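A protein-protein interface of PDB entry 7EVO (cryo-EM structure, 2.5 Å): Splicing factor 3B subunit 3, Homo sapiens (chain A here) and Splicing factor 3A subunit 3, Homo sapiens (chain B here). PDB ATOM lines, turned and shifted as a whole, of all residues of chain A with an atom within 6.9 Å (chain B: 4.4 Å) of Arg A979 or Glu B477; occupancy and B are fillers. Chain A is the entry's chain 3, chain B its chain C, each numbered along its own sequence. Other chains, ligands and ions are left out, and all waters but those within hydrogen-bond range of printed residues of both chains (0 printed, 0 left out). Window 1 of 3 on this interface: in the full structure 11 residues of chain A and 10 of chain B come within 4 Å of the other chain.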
ATOM      1  N   GLU A 946      17.642  -5.852  -9.370  1.00  0.00           N
ATOM      2  CA  GLU A 946      17.997  -7.192  -8.922  1.00  0.00           C
ATOM      3  C   GLU A 946      19.032  -7.872  -9.806  1.00  0.00           C
ATOM      4  O   GLU A 946      19.262  -9.075  -9.646  1.00  0.00           O
ATOM      5  CB  GLU A 946      16.741  -8.064  -8.843  1.00  0.00           C
ATOM      6  CG  GLU A 946      15.928  -8.118 -10.128  1.00  0.00           C
ATOM      7  CD  GLU A 946      14.900  -7.005 -10.233  1.00  0.00           C
ATOM      8  OE1 GLU A 946      15.134  -5.909  -9.679  1.00  0.00           O
ATOM      9  OE2 GLU A 946      13.852  -7.227 -10.872  1.00  0.00           O
ATOM     10  N   ARG A 968      13.331  -3.317 -19.694  1.00  0.00           N
ATOM     11  CA  ARG A 968      12.368  -2.494 -18.979  1.00  0.00           C
ATOM     12  C   ARG A 968      12.362  -1.076 -19.529  1.00  0.00           C
ATOM     13  O   ARG A 968      13.359  -0.582 -20.062  1.00  0.00           O
ATOM     14  CB  ARG A 968      12.669  -2.467 -17.474  1.00  0.00           C
ATOM     15  CG  ARG A 968      12.358  -3.762 -16.755  1.00  0.00           C
ATOM     16  CD  ARG A 968      12.907  -3.740 -15.348  1.00  0.00           C
ATOM     17  NE  ARG A 968      12.467  -4.888 -14.568  1.00  0.00           N
ATOM     18  CZ  ARG A 968      12.934  -5.190 -13.362  1.00  0.00           C
ATOM     19  NH1 ARG A 968      13.857  -4.425 -12.797  1.00  0.00           N
ATOM     20  NH2 ARG A 968      12.478  -6.254 -12.722  1.00  0.00           N
ATOM     21  N   VAL A 969      11.211  -0.421 -19.383  1.00  0.00           N
ATOM     22  CA  VAL A 969      11.040   0.999 -19.668  1.00  0.00           C
ATOM     23  C   VAL A 969      10.993   1.705 -18.319  1.00  0.00           C
ATOM     24  O   VAL A 969      10.388   1.192 -17.370  1.00  0.00           O
ATOM     25  CB  VAL A 969       9.772   1.284 -20.484  1.00  0.00           C
ATOM     26  CG1 VAL A 969       9.610   2.772 -20.714  1.00  0.00           C
ATOM     27  CG2 VAL A 969       9.815   0.551 -21.810  1.00  0.00           C
ATOM     28  N   TYR A 970      11.626   2.867 -18.229  1.00  0.00           N
ATOM     29  CA  TYR A 970      11.757   3.611 -16.985  1.00  0.00           C
ATOM     30  C   TYR A 970      11.500   5.093 -17.233  1.00  0.00           C
ATOM     31  O   TYR A 970      12.046   5.697 -18.158  1.00  0.00           O
ATOM     32  CB  TYR A 970      13.147   3.408 -16.377  1.00  0.00           C
ATOM     33  CG  TYR A 970      13.270   2.226 -15.450  1.00  0.00           C
ATOM     34  CD1 TYR A 970      12.678   2.239 -14.198  1.00  0.00           C
ATOM     35  CD2 TYR A 970      13.988   1.098 -15.823  1.00  0.00           C
ATOM     36  CE1 TYR A 970      12.793   1.163 -13.344  1.00  0.00           C
ATOM     37  CE2 TYR A 970      14.108   0.017 -14.977  1.00  0.00           C
ATOM     38  CZ  TYR A 970      13.508   0.056 -13.739  1.00  0.00           C
ATOM     39  OH  TYR A 970      13.625  -1.019 -12.893  1.00  0.00           O
ATOM     40  N   ASP A 971      10.659   5.684 -16.389  1.00  0.00           N
ATOM     41  CA  ASP A 971      10.436   7.122 -16.428  1.00  0.00           C
ATOM     42  C   ASP A 971      11.068   7.738 -15.189  1.00  0.00           C
ATOM     43  O   ASP A 971      11.269   7.065 -14.176  1.00  0.00           O
ATOM     44  CB  ASP A 971       8.944   7.458 -16.509  1.00  0.00           C
ATOM     45  CG  ASP A 971       8.691   8.874 -16.991  1.00  0.00           C
ATOM     46  OD1 ASP A 971       9.667   9.629 -17.184  1.00  0.00           O
ATOM     47  OD2 ASP A 971       7.510   9.235 -17.182  1.00  0.00           O
ATOM     48  N   LYS A 976      13.008   8.021  -7.305  1.00  0.00           N
ATOM     49  CA  LYS A 976      13.624   6.883  -7.978  1.00  0.00           C
ATOM     50  C   LYS A 976      13.093   6.828  -9.408  1.00  0.00           C
ATOM     51  O   LYS A 976      12.346   7.714  -9.836  1.00  0.00           O
ATOM     52  CB  LYS A 976      13.359   5.583  -7.200  1.00  0.00           C
ATOM     53  CG  LYS A 976      11.899   5.176  -7.141  1.00  0.00           C
ATOM     54  CD  LYS A 976      11.756   3.774  -6.581  1.00  0.00           C
ATOM     55  CE  LYS A 976      10.321   3.285  -6.664  1.00  0.00           C
ATOM     56  NZ  LYS A 976      10.158   1.943  -6.039  1.00  0.00           N
ATOM     57  N   LEU A 977      13.483   5.797 -10.147  1.00  0.00           N
ATOM     58  CA  LEU A 977      12.985   5.564 -11.492  1.00  0.00           C
ATOM     59  C   LEU A 977      11.798   4.609 -11.449  1.00  0.00           C
ATOM     60  O   LEU A 977      11.804   3.601 -10.739  1.00  0.00           O
ATOM     61  CB  LEU A 977      14.087   5.002 -12.393  1.00  0.00           C
ATOM     62  CG  LEU A 977      15.306   5.896 -12.626  1.00  0.00           C
ATOM     63  CD1 LEU A 977      16.428   5.101 -13.256  1.00  0.00           C
ATOM     64  CD2 LEU A 977      14.942   7.083 -13.496  1.00  0.00           C
ATOM     65  N   LEU A 978      10.773   4.943 -12.224  1.00  0.00           N
ATOM     66  CA  LEU A 978       9.483   4.259 -12.174  1.00  0.00           C
ATOM     67  C   LEU A 978       9.401   3.276 -13.337  1.00  0.00           C
ATOM     68  O   LEU A 978       9.489   3.673 -14.502  1.00  0.00           O
ATOM     69  CB  LEU A 978       8.342   5.269 -12.216  1.00  0.00           C
ATOM     70  CG  LEU A 978       8.371   6.324 -11.110  1.00  0.00           C
ATOM     71  CD1 LEU A 978       7.357   7.414 -11.389  1.00  0.00           C
ATOM     72  CD2 LEU A 978       8.124   5.692  -9.753  1.00  0.00           C
ATOM     73  N   ARG A 979       9.234   1.996 -13.017  1.00  0.00           N
ATOM     74  CA  ARG A 979       9.092   0.967 -14.039  1.00  0.00           C
ATOM     75  C   ARG A 979       7.745   1.112 -14.735  1.00  0.00           C
ATOM     76  O   ARG A 979       6.710   1.251 -14.077  1.00  0.00           O
ATOM     77  CB  ARG A 979       9.231  -0.416 -13.413  1.00  0.00           C
ATOM     78  CG  ARG A 979       9.089  -1.554 -14.403  1.00  0.00           C
ATOM     79  CD  ARG A 979       9.733  -2.822 -13.882  1.00  0.00           C
ATOM     80  NE  ARG A 979       8.806  -3.645 -13.115  1.00  0.00           N
ATOM     81  CZ  ARG A 979       8.851  -3.791 -11.796  1.00  0.00           C
ATOM     82  NH1 ARG A 979       9.782  -3.165 -11.089  1.00  0.00           N
ATOM     83  NH2 ARG A 979       7.968  -4.564 -11.183  1.00  0.00           N
ATOM     84  N   LYS A 980       7.755   1.070 -16.066  1.00  0.00           N
ATOM     85  CA  LYS A 980       6.569   1.344 -16.867  1.00  0.00           C
ATOM     86  C   LYS A 980       6.152   0.164 -17.734  1.00  0.00           C
ATOM     87  O   LYS A 980       4.957  -0.092 -17.900  1.00  0.00           O
ATOM     88  CB  LYS A 980       6.809   2.576 -17.744  1.00  0.00           C
ATOM     89  CG  LYS A 980       6.778   3.884 -16.982  1.00  0.00           C
ATOM     90  CD  LYS A 980       5.380   4.192 -16.484  1.00  0.00           C
ATOM     91  CE  LYS A 980       5.358   5.455 -15.649  1.00  0.00           C
ATOM     92  NZ  LYS A 980       5.609   5.174 -14.214  1.00  0.00           N
ATOM     93  N   CYS A 981       7.115  -0.558 -18.301  1.00  0.00           N
ATOM     94  CA  CYS A 981       6.832  -1.711 -19.142  1.00  0.00           C
ATOM     95  C   CYS A 981       7.974  -2.704 -19.005  1.00  0.00           C
ATOM     96  O   CYS A 981       9.062  -2.363 -18.540  1.00  0.00           O
ATOM     97  CB  CYS A 981       6.640  -1.307 -20.610  1.00  0.00           C
ATOM     98  SG  CYS A 981       5.779  -2.529 -21.619  1.00  0.00           S
ATOM     99  N   GLU A 982       7.720  -3.942 -19.423  1.00  0.00           N
ATOM    100  CA  GLU A 982       8.706  -4.998 -19.235  1.00  0.00           C
ATOM    101  C   GLU A 982       8.433  -6.147 -20.192  1.00  0.00           C
ATOM    102  O   GLU A 982       7.282  -6.559 -20.360  1.00  0.00           O
ATOM    103  CB  GLU A 982       8.690  -5.497 -17.787  1.00  0.00           C
ATOM    104  CG  GLU A 982       9.560  -6.708 -17.536  1.00  0.00           C
ATOM    105  CD  GLU A 982       9.759  -6.981 -16.061  1.00  0.00           C
ATOM    106  OE1 GLU A 982       9.047  -6.369 -15.239  1.00  0.00           O
ATOM    107  OE2 GLU A 982      10.621  -7.813 -15.719  1.00  0.00           O
ATOM    108  N   ASN A1019       1.059  -0.116 -24.314  1.00  0.00           N
ATOM    109  CA  ASN A1019       2.116  -0.243 -23.310  1.00  0.00           C
ATOM    110  C   ASN A1019       2.645  -1.681 -23.261  1.00  0.00           C
ATOM    111  O   ASN A1019       2.600  -2.365 -22.238  1.00  0.00           O
ATOM    112  CB  ASN A1019       1.618   0.216 -21.934  1.00  0.00           C
ATOM    113  CG  ASN A1019       2.744   0.639 -21.017  1.00  0.00           C
ATOM    114  OD1 ASN A1019       3.610   1.425 -21.398  1.00  0.00           O
ATOM    115  ND2 ASN A1019       2.743   0.114 -19.800  1.00  0.00           N
ATOM    116  N   TRP B 471       3.430  -9.957 -18.596  1.00  0.00           N
ATOM    117  CA  TRP B 471       3.551  -8.602 -18.072  1.00  0.00           C
ATOM    118  C   TRP B 471       2.186  -8.155 -17.562  1.00  0.00           C
ATOM    119  O   TRP B 471       1.287  -7.864 -18.359  1.00  0.00           O
ATOM    120  CB  TRP B 471       4.066  -7.646 -19.150  1.00  0.00           C
ATOM    121  CG  TRP B 471       3.773  -6.195 -18.881  1.00  0.00           C
ATOM    122  CD1 TRP B 471       2.935  -5.385 -19.591  1.00  0.00           C
ATOM    123  CD2 TRP B 471       4.333  -5.380 -17.845  1.00  0.00           C
ATOM    124  NE1 TRP B 471       2.930  -4.122 -19.055  1.00  0.00           N
ATOM    125  CE2 TRP B 471       3.777  -4.092 -17.980  1.00  0.00           C
ATOM    126  CE3 TRP B 471       5.240  -5.616 -16.809  1.00  0.00           C
ATOM    127  CZ2 TRP B 471       4.103  -3.047 -17.124  1.00  0.00           C
ATOM    128  CZ3 TRP B 471       5.563  -4.574 -15.961  1.00  0.00           C
ATOM    129  CH2 TRP B 471       4.999  -3.304 -16.126  1.00  0.00           C
ATOM    130  N   PRO B 473       0.392  -5.279 -15.851  1.00  0.00           N
ATOM    131  CA  PRO B 473       0.624  -3.885 -15.437  1.00  0.00           C
ATOM    132  C   PRO B 473      -0.071  -3.496 -14.142  1.00  0.00           C
ATOM    133  O   PRO B 473       0.388  -2.572 -13.459  1.00  0.00           O
ATOM    134  CB  PRO B 473       0.092  -3.081 -16.632  1.00  0.00           C
ATOM    135  CG  PRO B 473      -0.903  -3.979 -17.277  1.00  0.00           C
ATOM    136  CD  PRO B 473      -0.384  -5.372 -17.097  1.00  0.00           C
ATOM    137  N   THR B 475      -0.427  -4.993 -11.118  1.00  0.00           N
ATOM    138  CA  THR B 475       0.385  -5.155  -9.916  1.00  0.00           C
ATOM    139  C   THR B 475       1.840  -4.787 -10.187  1.00  0.00           C
ATOM    140  O   THR B 475       2.576  -4.391  -9.275  1.00  0.00           O
ATOM    141  CB  THR B 475       0.272  -6.589  -9.389  1.00  0.00           C
ATOM    142  OG1 THR B 475       1.316  -6.835  -8.440  1.00  0.00           O
ATOM    143  CG2 THR B 475       0.372  -7.600 -10.525  1.00  0.00           C
ATOM    144  N   GLU B 476       2.270  -4.905 -11.439  1.00  0.00           N
ATOM    145  CA  GLU B 476       3.613  -4.520 -11.846  1.00  0.00           C
ATOM    146  C   GLU B 476       3.562  -3.159 -12.518  1.00  0.00           C
ATOM    147  O   GLU B 476       3.308  -3.070 -13.723  1.00  0.00           O
ATOM    148  CB  GLU B 476       4.217  -5.548 -12.799  1.00  0.00           C
ATOM    149  CG  GLU B 476       5.075  -6.594 -12.135  1.00  0.00           C
ATOM    150  CD  GLU B 476       5.495  -7.677 -13.100  1.00  0.00           C
ATOM    151  OE1 GLU B 476       4.618  -8.428 -13.574  1.00  0.00           O
ATOM    152  OE2 GLU B 476       6.702  -7.771 -13.399  1.00  0.00           O
ATOM    153  N   GLU B 477       3.783  -2.108 -11.733  1.00  0.00           N
ATOM    154  CA  GLU B 477       3.916  -0.748 -12.237  1.00  0.00           C
ATOM    155  C   GLU B 477       4.309   0.157 -11.081  1.00  0.00           C
ATOM    156  O   GLU B 477       4.001  -0.140  -9.922  1.00  0.00           O
ATOM    157  CB  GLU B 477       2.621  -0.259 -12.890  1.00  0.00           C
ATOM    158  CG  GLU B 477       2.809   0.913 -13.836  1.00  0.00           C
ATOM    159  CD  GLU B 477       2.192   0.662 -15.193  1.00  0.00           C
ATOM    160  OE1 GLU B 477       2.046   1.624 -15.974  1.00  0.00           O
ATOM    161  OE2 GLU B 477       1.858  -0.504 -15.480  1.00  0.00           O
ATOM    162  N   GLU B 478       4.982   1.262 -11.379  1.00  0.00           N
ATOM    163  CA  GLU B 478       5.458   2.188 -10.357  1.00  0.00           C
ATOM    164  C   GLU B 478       4.866   3.559 -10.659  1.00  0.00           C
ATOM    165  O   GLU B 478       5.344   4.268 -11.549  1.00  0.00           O
ATOM    166  CB  GLU B 478       6.981   2.233 -10.317  1.00  0.00           C
ATOM    167  N   TYR B 479       3.811   3.916  -9.934  1.00  0.00           N
ATOM    168  CA  TYR B 479       3.256   5.256 -10.010  1.00  0.00           C
ATOM    169  C   TYR B 479       3.627   6.030  -8.753  1.00  0.00           C
ATOM    170  O   TYR B 479       3.740   5.451  -7.669  1.00  0.00           O
ATOM    171  CB  TYR B 479       1.738   5.202 -10.177  1.00  0.00           C
ATOM    172  N   THR B 491       3.161   3.459  -4.851  1.00  0.00           N
ATOM    173  CA  THR B 491       1.760   3.336  -5.228  1.00  0.00           C
ATOM    174  C   THR B 491       1.612   2.370  -6.398  1.00  0.00           C
ATOM    175  O   THR B 491       2.342   2.467  -7.389  1.00  0.00           O
ATOM    176  CB  THR B 491       1.189   4.705  -5.591  1.00  0.00           C
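The backbone carbonyl oxygen (O) of Arg A979 is in hydrogen-bond range of the backbone NH (N) of Glu B478 (3.2 Å). The side-chain amino group of Lys A980 is in hydrogen-bond range of the backbone carbonyl oxygen of Glu B478. The side-chain carboxylate (OE1) of Glu A982 lies close to the side-chain carboxylate (OE2) of Glu B476 (3.3 Å).
NE of Arg A968 lies within salt-bridge range of OE2 of Glu A982 (3.6 Å). N of Lys A980 is in hydrogen-bond range of O of Val A969 (2.9 Å). The backbone NH (N) of Val A969 is in hydrogen-bond range of the backbone carbonyl oxygen (O) of Cys A981 (3.0 Å). The backbone NH (N) of Leu A978 sits at hydrogen-bond distance from the backbone carbonyl oxygen (O) of Asp A971, 2.9 Å away. The side-chain amide nitrogen (ND2) of Asn A1019 sits at hydrogen-bond distance from the backbone carbonyl oxygen (O) of Lys A980, at 2.9 Å. O of Asn A1019 is in hydrogen-bond range of SG of Cys A981, 3.2 Å away.
Of the 13 printed residues of chain A, 6 touch a printed residue of chain B. Hydrophobic or aromatic side chains of chain A within 4 Å of the printed part of chain B: Leu A978. Along chain A the printed residues that touch a printed residue of chain B span positions 978 to 1019. Of the 8 printed residues of chain B, 4 touch a printed residue of chain A. Hydrophobic or aromatic side chains of chain B that line the printed part of chain A: Trp B471. Among the printed residues, no Asp or Glu carboxylate lies within 4 Å of a Lys or Arg side-chain nitrogen of the other chain.
Arg A979 touches just these residues of chain B: Glu B476 (3.7 Å), Glu B477 (3.9 Å) and Glu B478 (3.2 Å). Of the printed residues of chain B, Lys A980 touches Trp B471, Glu B477 and Glu B478. Printed residues of chain B within 4 Å of Glu A982: Trp B471 (3.6 Å) and Glu B476 (3.3 Å). Of chain A, only Arg A979 and Lys A980 come within 4 Å of Glu B477. Of the printed residues of chain A, Glu B478 touches Leu A978 (3.2 Å), Arg A979 (3.2 Å) and Lys A980 (2.8 Å). The nearest printed residue of chain B that does not touch Arg A979 is Trp B471 (4.4 Å).
Among the printed residues, merely in contact across the chains: Leu A978 with Glu B478 (3.2 Å), Arg A979 with Glu B476 (3.7 Å), Arg A979 with Glu B477 (3.9 Å), Lys A980 with Trp B471 (3.2 Å), Lys A980 with Glu B477 (3.9 Å), Cys A981 with Trp B471 (3.6 Å), Glu A982 with Trp B471 (3.6 Å) and Asn A1019 with Trp B471 (3.7 Å).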
